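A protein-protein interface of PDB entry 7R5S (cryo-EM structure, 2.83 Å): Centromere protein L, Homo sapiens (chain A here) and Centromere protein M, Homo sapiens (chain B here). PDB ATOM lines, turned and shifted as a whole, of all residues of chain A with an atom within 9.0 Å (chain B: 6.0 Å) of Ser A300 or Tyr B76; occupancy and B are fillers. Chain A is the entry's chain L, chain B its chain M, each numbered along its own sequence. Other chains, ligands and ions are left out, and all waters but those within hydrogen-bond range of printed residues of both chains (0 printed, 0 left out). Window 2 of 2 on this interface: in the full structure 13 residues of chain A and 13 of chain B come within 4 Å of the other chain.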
ATOM      1  N   ALA A 215      -0.990 -29.219  13.843  1.00  0.00           N
ATOM      2  CA  ALA A 215      -1.532 -28.519  12.683  1.00  0.00           C
ATOM      3  C   ALA A 215      -2.728 -29.247  12.083  1.00  0.00           C
ATOM      4  O   ALA A 215      -3.593 -28.611  11.472  1.00  0.00           O
ATOM      5  CB  ALA A 215      -0.442 -28.331  11.628  1.00  0.00           C
ATOM      6  N   TRP A 241       1.366 -18.736  10.308  1.00  0.00           N
ATOM      7  CA  TRP A 241       2.264 -19.766   9.805  1.00  0.00           C
ATOM      8  C   TRP A 241       3.697 -19.450  10.206  1.00  0.00           C
ATOM      9  O   TRP A 241       4.116 -18.287  10.188  1.00  0.00           O
ATOM     10  CB  TRP A 241       2.172 -19.887   8.280  1.00  0.00           C
ATOM     11  CG  TRP A 241       1.049 -20.753   7.803  1.00  0.00           C
ATOM     12  CD1 TRP A 241       1.001 -22.116   7.816  1.00  0.00           C
ATOM     13  CD2 TRP A 241      -0.188 -20.315   7.230  1.00  0.00           C
ATOM     14  NE1 TRP A 241      -0.189 -22.555   7.292  1.00  0.00           N
ATOM     15  CE2 TRP A 241      -0.938 -21.468   6.925  1.00  0.00           C
ATOM     16  CE3 TRP A 241      -0.737 -19.060   6.948  1.00  0.00           C
ATOM     17  CZ2 TRP A 241      -2.206 -21.404   6.351  1.00  0.00           C
ATOM     18  CZ3 TRP A 241      -1.993 -18.999   6.378  1.00  0.00           C
ATOM     19  CH2 TRP A 241      -2.714 -20.163   6.087  1.00  0.00           C
ATOM     20  N   SER A 242       4.444 -20.492  10.560  1.00  0.00           N
ATOM     21  CA  SER A 242       5.854 -20.381  10.914  1.00  0.00           C
ATOM     22  C   SER A 242       6.681 -21.059   9.831  1.00  0.00           C
ATOM     23  O   SER A 242       6.602 -22.279   9.657  1.00  0.00           O
ATOM     24  CB  SER A 242       6.127 -21.013  12.279  1.00  0.00           C
ATOM     25  OG  SER A 242       7.445 -20.733  12.714  1.00  0.00           O
ATOM     26  N   VAL A 243       7.471 -20.270   9.111  1.00  0.00           N
ATOM     27  CA  VAL A 243       8.281 -20.777   8.005  1.00  0.00           C
ATOM     28  C   VAL A 243       9.550 -21.411   8.563  1.00  0.00           C
ATOM     29  O   VAL A 243      10.307 -20.743   9.281  1.00  0.00           O
ATOM     30  CB  VAL A 243       8.619 -19.659   7.006  1.00  0.00           C
ATOM     31  CG1 VAL A 243       9.410 -20.218   5.836  1.00  0.00           C
ATOM     32  CG2 VAL A 243       7.349 -18.979   6.524  1.00  0.00           C
ATOM     33  N   PRO A 244       9.826 -22.684   8.265  1.00  0.00           N
ATOM     34  CA  PRO A 244      11.063 -23.295   8.767  1.00  0.00           C
ATOM     35  C   PRO A 244      12.287 -22.810   8.008  1.00  0.00           C
ATOM     36  O   PRO A 244      12.561 -23.249   6.886  1.00  0.00           O
ATOM     37  CB  PRO A 244      10.822 -24.794   8.558  1.00  0.00           C
ATOM     38  CG  PRO A 244       9.862 -24.861   7.420  1.00  0.00           C
ATOM     39  CD  PRO A 244       8.985 -23.644   7.530  1.00  0.00           C
ATOM     40  N   MET A 284      -8.123 -25.678   2.188  1.00  0.00           N
ATOM     41  CA  MET A 284      -6.762 -25.213   2.435  1.00  0.00           C
ATOM     42  C   MET A 284      -6.002 -24.976   1.134  1.00  0.00           C
ATOM     43  O   MET A 284      -5.195 -24.041   1.043  1.00  0.00           O
ATOM     44  CB  MET A 284      -6.018 -26.215   3.317  1.00  0.00           C
ATOM     45  CG  MET A 284      -6.415 -26.156   4.780  1.00  0.00           C
ATOM     46  SD  MET A 284      -6.145 -24.525   5.498  1.00  0.00           S
ATOM     47  CE  MET A 284      -6.776 -24.773   7.153  1.00  0.00           C
ATOM     48  N   ASP A 285      -6.249 -25.806   0.117  1.00  0.00           N
ATOM     49  CA  ASP A 285      -5.564 -25.641  -1.159  1.00  0.00           C
ATOM     50  C   ASP A 285      -5.982 -24.356  -1.858  1.00  0.00           C
ATOM     51  O   ASP A 285      -5.178 -23.759  -2.580  1.00  0.00           O
ATOM     52  CB  ASP A 285      -5.832 -26.845  -2.061  1.00  0.00           C
ATOM     53  CG  ASP A 285      -4.838 -27.967  -1.842  1.00  0.00           C
ATOM     54  OD1 ASP A 285      -4.589 -28.736  -2.794  1.00  0.00           O
ATOM     55  OD2 ASP A 285      -4.306 -28.082  -0.718  1.00  0.00           O
ATOM     56  N   LEU A 287      -6.605 -21.431  -0.377  1.00  0.00           N
ATOM     57  CA  LEU A 287      -5.766 -20.391   0.209  1.00  0.00           C
ATOM     58  C   LEU A 287      -4.309 -20.552  -0.210  1.00  0.00           C
ATOM     59  O   LEU A 287      -3.619 -19.558  -0.469  1.00  0.00           O
ATOM     60  CB  LEU A 287      -5.888 -20.414   1.731  1.00  0.00           C
ATOM     61  CG  LEU A 287      -7.297 -20.261   2.308  1.00  0.00           C
ATOM     62  CD1 LEU A 287      -7.270 -20.394   3.821  1.00  0.00           C
ATOM     63  CD2 LEU A 287      -7.905 -18.931   1.896  1.00  0.00           C
ATOM     64  N   TYR A 288      -3.824 -21.795  -0.279  1.00  0.00           N
ATOM     65  CA  TYR A 288      -2.448 -22.028  -0.712  1.00  0.00           C
ATOM     66  C   TYR A 288      -2.215 -21.480  -2.115  1.00  0.00           C
ATOM     67  O   TYR A 288      -1.220 -20.790  -2.370  1.00  0.00           O
ATOM     68  CB  TYR A 288      -2.126 -23.522  -0.660  1.00  0.00           C
ATOM     69  CG  TYR A 288      -2.031 -24.092   0.737  1.00  0.00           C
ATOM     70  CD1 TYR A 288      -1.836 -23.265   1.834  1.00  0.00           C
ATOM     71  CD2 TYR A 288      -2.132 -25.459   0.957  1.00  0.00           C
ATOM     72  CE1 TYR A 288      -1.747 -23.783   3.111  1.00  0.00           C
ATOM     73  CE2 TYR A 288      -2.045 -25.986   2.229  1.00  0.00           C
ATOM     74  CZ  TYR A 288      -1.853 -25.144   3.303  1.00  0.00           C
ATOM     75  OH  TYR A 288      -1.765 -25.665   4.573  1.00  0.00           O
ATOM     76  N   SER A 289      -3.134 -21.769  -3.039  1.00  0.00           N
ATOM     77  CA  SER A 289      -2.985 -21.295  -4.409  1.00  0.00           C
ATOM     78  C   SER A 289      -3.133 -19.781  -4.492  1.00  0.00           C
ATOM     79  O   SER A 289      -2.410 -19.125  -5.250  1.00  0.00           O
ATOM     80  CB  SER A 289      -4.003 -21.984  -5.317  1.00  0.00           C
ATOM     81  OG  SER A 289      -5.232 -21.280  -5.329  1.00  0.00           O
ATOM     82  N   PHE A 291      -2.298 -17.649  -2.245  1.00  0.00           N
ATOM     83  CA  PHE A 291      -1.073 -17.043  -1.732  1.00  0.00           C
ATOM     84  C   PHE A 291       0.086 -17.230  -2.705  1.00  0.00           C
ATOM     85  O   PHE A 291       0.905 -16.320  -2.889  1.00  0.00           O
ATOM     86  CB  PHE A 291      -0.730 -17.633  -0.365  1.00  0.00           C
ATOM     87  CG  PHE A 291       0.325 -16.869   0.381  1.00  0.00           C
ATOM     88  CD1 PHE A 291       1.665 -17.189   0.237  1.00  0.00           C
ATOM     89  CD2 PHE A 291      -0.022 -15.835   1.232  1.00  0.00           C
ATOM     90  CE1 PHE A 291       2.637 -16.489   0.924  1.00  0.00           C
ATOM     91  CE2 PHE A 291       0.946 -15.132   1.921  1.00  0.00           C
ATOM     92  CZ  PHE A 291       2.277 -15.459   1.767  1.00  0.00           C
ATOM     93  N   HIS A 292       0.176 -18.406  -3.334  1.00  0.00           N
ATOM     94  CA  HIS A 292       1.282 -18.670  -4.247  1.00  0.00           C
ATOM     95  C   HIS A 292       1.160 -17.862  -5.533  1.00  0.00           C
ATOM     96  O   HIS A 292       2.180 -17.512  -6.138  1.00  0.00           O
ATOM     97  CB  HIS A 292       1.359 -20.162  -4.567  1.00  0.00           C
ATOM     98  CG  HIS A 292       2.483 -20.523  -5.488  1.00  0.00           C
ATOM     99  ND1 HIS A 292       2.345 -20.546  -6.859  1.00  0.00           N
ATOM    100  CD2 HIS A 292       3.767 -20.872  -5.234  1.00  0.00           C
ATOM    101  CE1 HIS A 292       3.493 -20.896  -7.409  1.00  0.00           C
ATOM    102  NE2 HIS A 292       4.373 -21.099  -6.445  1.00  0.00           N
ATOM    103  N   ILE A 297       5.352 -18.243  -2.915  1.00  0.00           N
ATOM    104  CA  ILE A 297       5.854 -18.944  -1.739  1.00  0.00           C
ATOM    105  C   ILE A 297       4.945 -20.132  -1.466  1.00  0.00           C
ATOM    106  O   ILE A 297       3.720 -19.980  -1.389  1.00  0.00           O
ATOM    107  CB  ILE A 297       5.929 -18.014  -0.516  1.00  0.00           C
ATOM    108  CG1 ILE A 297       6.926 -16.881  -0.766  1.00  0.00           C
ATOM    109  CG2 ILE A 297       6.314 -18.796   0.729  1.00  0.00           C
ATOM    110  CD1 ILE A 297       7.057 -15.918   0.390  1.00  0.00           C
ATOM    111  N   HIS A 298       5.543 -21.312  -1.322  1.00  0.00           N
ATOM    112  CA  HIS A 298       4.790 -22.536  -1.058  1.00  0.00           C
ATOM    113  C   HIS A 298       4.384 -22.551   0.410  1.00  0.00           C
ATOM    114  O   HIS A 298       5.187 -22.873   1.287  1.00  0.00           O
ATOM    115  CB  HIS A 298       5.617 -23.766  -1.418  1.00  0.00           C
ATOM    116  CG  HIS A 298       5.919 -23.881  -2.878  1.00  0.00           C
ATOM    117  ND1 HIS A 298       4.949 -24.143  -3.820  1.00  0.00           N
ATOM    118  CD2 HIS A 298       7.085 -23.771  -3.559  1.00  0.00           C
ATOM    119  CE1 HIS A 298       5.503 -24.189  -5.018  1.00  0.00           C
ATOM    120  NE2 HIS A 298       6.798 -23.967  -4.888  1.00  0.00           N
ATOM    121  N   LEU A 299       3.127 -22.199   0.680  1.00  0.00           N
ATOM    122  CA  LEU A 299       2.627 -22.181   2.048  1.00  0.00           C
ATOM    123  C   LEU A 299       2.350 -23.575   2.592  1.00  0.00           C
ATOM    124  O   LEU A 299       2.092 -23.711   3.794  1.00  0.00           O
ATOM    125  CB  LEU A 299       1.357 -21.333   2.126  1.00  0.00           C
ATOM    126  CG  LEU A 299       1.180 -20.469   3.374  1.00  0.00           C
ATOM    127  CD1 LEU A 299       2.333 -19.491   3.516  1.00  0.00           C
ATOM    128  CD2 LEU A 299      -0.146 -19.732   3.323  1.00  0.00           C
ATOM    129  N   SER A 300       2.397 -24.608   1.748  1.00  0.00           N
ATOM    130  CA  SER A 300       2.171 -25.973   2.206  1.00  0.00           C
ATOM    131  C   SER A 300       3.385 -26.564   2.910  1.00  0.00           C
ATOM    132  O   SER A 300       3.249 -27.583   3.594  1.00  0.00           O
ATOM    133  CB  SER A 300       1.772 -26.863   1.027  1.00  0.00           C
ATOM    134  OG  SER A 300       2.593 -26.618  -0.100  1.00  0.00           O
ATOM    135  N   ALA A 301       4.558 -25.957   2.756  1.00  0.00           N
ATOM    136  CA  ALA A 301       5.772 -26.426   3.408  1.00  0.00           C
ATOM    137  C   ALA A 301       5.997 -25.792   4.775  1.00  0.00           C
ATOM    138  O   ALA A 301       7.009 -26.089   5.418  1.00  0.00           O
ATOM    139  CB  ALA A 301       6.987 -26.161   2.513  1.00  0.00           C
ATOM    140  N   THR A 302       5.090 -24.936   5.231  1.00  0.00           N
ATOM    141  CA  THR A 302       5.213 -24.266   6.514  1.00  0.00           C
ATOM    142  C   THR A 302       4.391 -25.007   7.567  1.00  0.00           C
ATOM    143  O   THR A 302       3.826 -26.074   7.312  1.00  0.00           O
ATOM    144  CB  THR A 302       4.785 -22.803   6.384  1.00  0.00           C
ATOM    145  OG1 THR A 302       3.418 -22.739   5.962  1.00  0.00           O
ATOM    146  CG2 THR A 302       5.655 -22.084   5.366  1.00  0.00           C
ATOM    147  N   ARG A 303       4.317 -24.436   8.766  1.00  0.00           N
ATOM    148  CA  ARG A 303       3.625 -25.044   9.894  1.00  0.00           C
ATOM    149  C   ARG A 303       2.564 -24.090  10.422  1.00  0.00           C
ATOM    150  O   ARG A 303       2.868 -22.937  10.747  1.00  0.00           O
ATOM    151  CB  ARG A 303       4.611 -25.406  11.009  1.00  0.00           C
ATOM    152  CG  ARG A 303       3.956 -25.930  12.274  1.00  0.00           C
ATOM    153  CD  ARG A 303       4.923 -25.904  13.444  1.00  0.00           C
ATOM    154  NE  ARG A 303       4.290 -26.334  14.687  1.00  0.00           N
ATOM    155  CZ  ARG A 303       4.853 -26.230  15.886  1.00  0.00           C
ATOM    156  NH1 ARG A 303       6.063 -25.704  16.009  1.00  0.00           N
ATOM    157  NH2 ARG A 303       4.204 -26.650  16.963  1.00  0.00           N
ATOM    158  N   LEU A 304       1.326 -24.571  10.507  1.00  0.00           N
ATOM    159  CA  LEU A 304       0.243 -23.770  11.060  1.00  0.00           C
ATOM    160  C   LEU A 304       0.378 -23.690  12.576  1.00  0.00           C
ATOM    161  O   LEU A 304       0.592 -24.706  13.245  1.00  0.00           O
ATOM    162  CB  LEU A 304      -1.107 -24.370  10.672  1.00  0.00           C
ATOM    163  CG  LEU A 304      -2.363 -23.589  11.057  1.00  0.00           C
ATOM    164  CD1 LEU A 304      -2.362 -22.217  10.410  1.00  0.00           C
ATOM    165  CD2 LEU A 304      -3.609 -24.365  10.665  1.00  0.00           C
ATOM    166  N   THR B  23      12.431 -33.917  -0.811  1.00  0.00           N
ATOM    167  CA  THR B  23      12.394 -32.469  -0.979  1.00  0.00           C
ATOM    168  C   THR B  23      13.463 -31.758  -0.157  1.00  0.00           C
ATOM    169  O   THR B  23      14.010 -30.743  -0.603  1.00  0.00           O
ATOM    170  CB  THR B  23      11.012 -31.926  -0.607  1.00  0.00           C
ATOM    171  OG1 THR B  23      10.662 -32.367   0.712  1.00  0.00           O
ATOM    172  CG2 THR B  23       9.964 -32.412  -1.595  1.00  0.00           C
ATOM    173  N   LYS B  50      15.151 -34.842  -6.484  1.00  0.00           N
ATOM    174  CA  LYS B  50      14.021 -34.152  -5.877  1.00  0.00           C
ATOM    175  C   LYS B  50      12.692 -34.807  -6.226  1.00  0.00           C
ATOM    176  O   LYS B  50      11.833 -34.968  -5.352  1.00  0.00           O
ATOM    177  CB  LYS B  50      14.008 -32.683  -6.309  1.00  0.00           C
ATOM    178  CG  LYS B  50      12.784 -31.910  -5.846  1.00  0.00           C
ATOM    179  CD  LYS B  50      12.796 -30.488  -6.379  1.00  0.00           C
ATOM    180  CE  LYS B  50      11.510 -29.757  -6.028  1.00  0.00           C
ATOM    181  NZ  LYS B  50      11.276 -29.716  -4.559  1.00  0.00           N
ATOM    182  N   HIS B  73       5.944 -33.234   8.453  1.00  0.00           N
ATOM    183  CA  HIS B  73       5.730 -31.855   8.866  1.00  0.00           C
ATOM    184  C   HIS B  73       5.367 -30.939   7.704  1.00  0.00           C
ATOM    185  O   HIS B  73       5.238 -29.727   7.903  1.00  0.00           O
ATOM    186  CB  HIS B  73       6.973 -31.320   9.579  1.00  0.00           C
ATOM    187  CG  HIS B  73       7.297 -32.038  10.852  1.00  0.00           C
ATOM    188  ND1 HIS B  73       8.450 -31.797  11.569  1.00  0.00           N
ATOM    189  CD2 HIS B  73       6.620 -32.988  11.538  1.00  0.00           C
ATOM    190  CE1 HIS B  73       8.470 -32.569  12.640  1.00  0.00           C
ATOM    191  NE2 HIS B  73       7.370 -33.302  12.645  1.00  0.00           N
ATOM    192  N   SER B  74       5.196 -31.484   6.501  1.00  0.00           N
ATOM    193  CA  SER B  74       4.881 -30.667   5.337  1.00  0.00           C
ATOM    194  C   SER B  74       4.098 -31.495   4.330  1.00  0.00           C
ATOM    195  O   SER B  74       4.483 -32.625   4.019  1.00  0.00           O
ATOM    196  CB  SER B  74       6.156 -30.115   4.691  1.00  0.00           C
ATOM    197  OG  SER B  74       6.687 -31.028   3.749  1.00  0.00           O
ATOM    198  N   LYS B  75       2.998 -30.928   3.828  1.00  0.00           N
ATOM    199  CA  LYS B  75       2.209 -31.586   2.794  1.00  0.00           C
ATOM    200  C   LYS B  75       2.852 -31.481   1.418  1.00  0.00           C
ATOM    201  O   LYS B  75       2.492 -32.249   0.518  1.00  0.00           O
ATOM    202  CB  LYS B  75       0.802 -30.989   2.746  1.00  0.00           C
ATOM    203  CG  LYS B  75       0.038 -31.096   4.053  1.00  0.00           C
ATOM    204  CD  LYS B  75      -1.461 -31.036   3.817  1.00  0.00           C
ATOM    205  CE  LYS B  75      -2.218 -30.836   5.118  1.00  0.00           C
ATOM    206  NZ  LYS B  75      -2.079 -29.445   5.630  1.00  0.00           N
ATOM    207  N   TYR B  76       3.787 -30.546   1.238  1.00  0.00           N
ATOM    208  CA  TYR B  76       4.469 -30.403  -0.043  1.00  0.00           C
ATOM    209  C   TYR B  76       5.245 -31.666  -0.396  1.00  0.00           C
ATOM    210  O   TYR B  76       5.220 -32.119  -1.546  1.00  0.00           O
ATOM    211  CB  TYR B  76       5.394 -29.187  -0.001  1.00  0.00           C
ATOM    212  CG  TYR B  76       5.998 -28.807  -1.332  1.00  0.00           C
ATOM    213  CD1 TYR B  76       5.210 -28.289  -2.351  1.00  0.00           C
ATOM    214  CD2 TYR B  76       7.359 -28.948  -1.564  1.00  0.00           C
ATOM    215  CE1 TYR B  76       5.760 -27.934  -3.567  1.00  0.00           C
ATOM    216  CE2 TYR B  76       7.916 -28.595  -2.776  1.00  0.00           C
ATOM    217  CZ  TYR B  76       7.113 -28.089  -3.774  1.00  0.00           C
ATOM    218  OH  TYR B  76       7.666 -27.737  -4.984  1.00  0.00           O
ATOM    219  N   SER B  77       5.927 -32.261   0.587  1.00  0.00           N
ATOM    220  CA  SER B  77       6.670 -33.490   0.334  1.00  0.00           C
ATOM    221  C   SER B  77       5.734 -34.647   0.009  1.00  0.00           C
ATOM    222  O   SER B  77       6.041 -35.478  -0.853  1.00  0.00           O
ATOM    223  CB  SER B  77       7.545 -33.830   1.539  1.00  0.00           C
ATOM    224  OG  SER B  77       6.790 -33.813   2.736  1.00  0.00           O
ATOM    225  N   LEU B  78       4.587 -34.718   0.689  1.00  0.00           N
ATOM    226  CA  LEU B  78       3.617 -35.766   0.389  1.00  0.00           C
ATOM    227  C   LEU B  78       3.082 -35.630  -1.030  1.00  0.00           C
ATOM    228  O   LEU B  78       2.968 -36.624  -1.756  1.00  0.00           O
ATOM    229  CB  LEU B  78       2.473 -35.730   1.402  1.00  0.00           C
ATOM    230  CG  LEU B  78       1.357 -36.754   1.191  1.00  0.00           C
ATOM    231  CD1 LEU B  78       1.904 -38.170   1.274  1.00  0.00           C
ATOM    232  CD2 LEU B  78       0.240 -36.550   2.201  1.00  0.00           C
ATOM    233  N   GLN B  79       2.751 -34.404  -1.444  1.00  0.00           N
ATOM    234  CA  GLN B  79       2.288 -34.189  -2.812  1.00  0.00           C
ATOM    235  C   GLN B  79       3.380 -34.526  -3.822  1.00  0.00           C
ATOM    236  O   GLN B  79       3.102 -35.106  -4.879  1.00  0.00           O
ATOM    237  CB  GLN B  79       1.820 -32.745  -2.989  1.00  0.00           C
ATOM    238  CG  GLN B  79       0.609 -32.377  -2.150  1.00  0.00           C
ATOM    239  CD  GLN B  79       0.243 -30.911  -2.269  1.00  0.00           C
ATOM    240  OE1 GLN B  79       0.846 -30.170  -3.045  1.00  0.00           O
ATOM    241  NE2 GLN B  79      -0.751 -30.485  -1.498  1.00  0.00           N
ATOM    242  N   ASN B  80       4.630 -34.178  -3.508  1.00  0.00           N
ATOM    243  CA  ASN B  80       5.735 -34.496  -4.406  1.00  0.00           C
ATOM    244  C   ASN B  80       5.903 -36.001  -4.565  1.00  0.00           C
ATOM    245  O   ASN B  80       6.113 -36.495  -5.679  1.00  0.00           O
ATOM    246  CB  ASN B  80       7.025 -33.860  -3.888  1.00  0.00           C
ATOM    247  CG  ASN B  80       8.199 -34.083  -4.818  1.00  0.00           C
ATOM    248  OD1 ASN B  80       8.395 -33.336  -5.776  1.00  0.00           O
ATOM    249  ND2 ASN B  80       8.989 -35.112  -4.538  1.00  0.00           N
ATOM    250  N   THR B  81       5.804 -36.750  -3.464  1.00  0.00           N
ATOM    251  CA  THR B  81       5.922 -38.203  -3.551  1.00  0.00           C
ATOM    252  C   THR B  81       4.745 -38.810  -4.306  1.00  0.00           C
ATOM    253  O   THR B  81       4.924 -39.745  -5.097  1.00  0.00           O
ATOM    254  CB  THR B  81       6.030 -38.813  -2.154  1.00  0.00           C
ATOM    255  OG1 THR B  81       4.939 -38.358  -1.345  1.00  0.00           O
ATOM    256  CG2 THR B  81       7.344 -38.416  -1.499  1.00  0.00           C
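Of the printed residues of chain B, Ser A300 touches Ser B74 (3.9 Å), Lys B75 (3.4 Å) and Tyr B76 (3.8 Å). Of chain A, only His A298 (3.9 Å) and Ser A300 (3.8 Å) come within 4 Å of Tyr B76. No residue of chain A comes within 4 Å of Ser B77. Printed residues of chain B within 4 Å of Tyr A288: Lys B75 (3.9 Å). Of the printed residues of chain A, Ser B74 touches Ser A300 (3.9 Å) and Ala A301 (3.9 Å). The nearest residue of chain B that does not touch Ser A300 is Gln B79 (4.9 Å). The nearest residue of chain A that does not touch Tyr B76 is Ala A301 (4.2 Å). The nearest printed residue of chain B that does not touch Ala A301 is Tyr B76 (4.2 Å).
NZ of Lys B75 touches OH of Tyr A288, 3.9 Å away. NE2 of His A298 touches OH of Tyr B76 (3.9 Å). Ser A300 touches Ser B74. OG of Ser A300 touches CB of Tyr B76 (3.8 Å). Ser B74 touches Ala A301 (CB to CA, 3.9 Å). O of Thr A302 touches O of His B73, 3.96 Å away.
Of the 11 printed residues of chain B, 4 touch a printed residue of chain A. Hydrophobic or aromatic side chains of chain B that line the printed part of chain A: Tyr B76. Printed residues of chain A that touch a printed residue of chain B: Tyr A288, His A298, Ser A300, Ala A301 and Thr A302. Among the printed residues, no Asp or Glu carboxylate lies within 4 Å of a Lys or Arg side-chain nitrogen of the other chain.
The backbone carbonyl oxygen (O) of Leu A299 is in hydrogen-bond range of the side-chain hydroxyl (OG1) of Thr A302, at 2.7 Å. The backbone carbonyl oxygen (O) of Ser B74 sits at hydrogen-bond distance from the side-chain hydroxyl (OG) of Ser B77, at 2.9 Å.
O of Ser A300 is in hydrogen-bond range of N of Lys B75 (3.4 Å).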
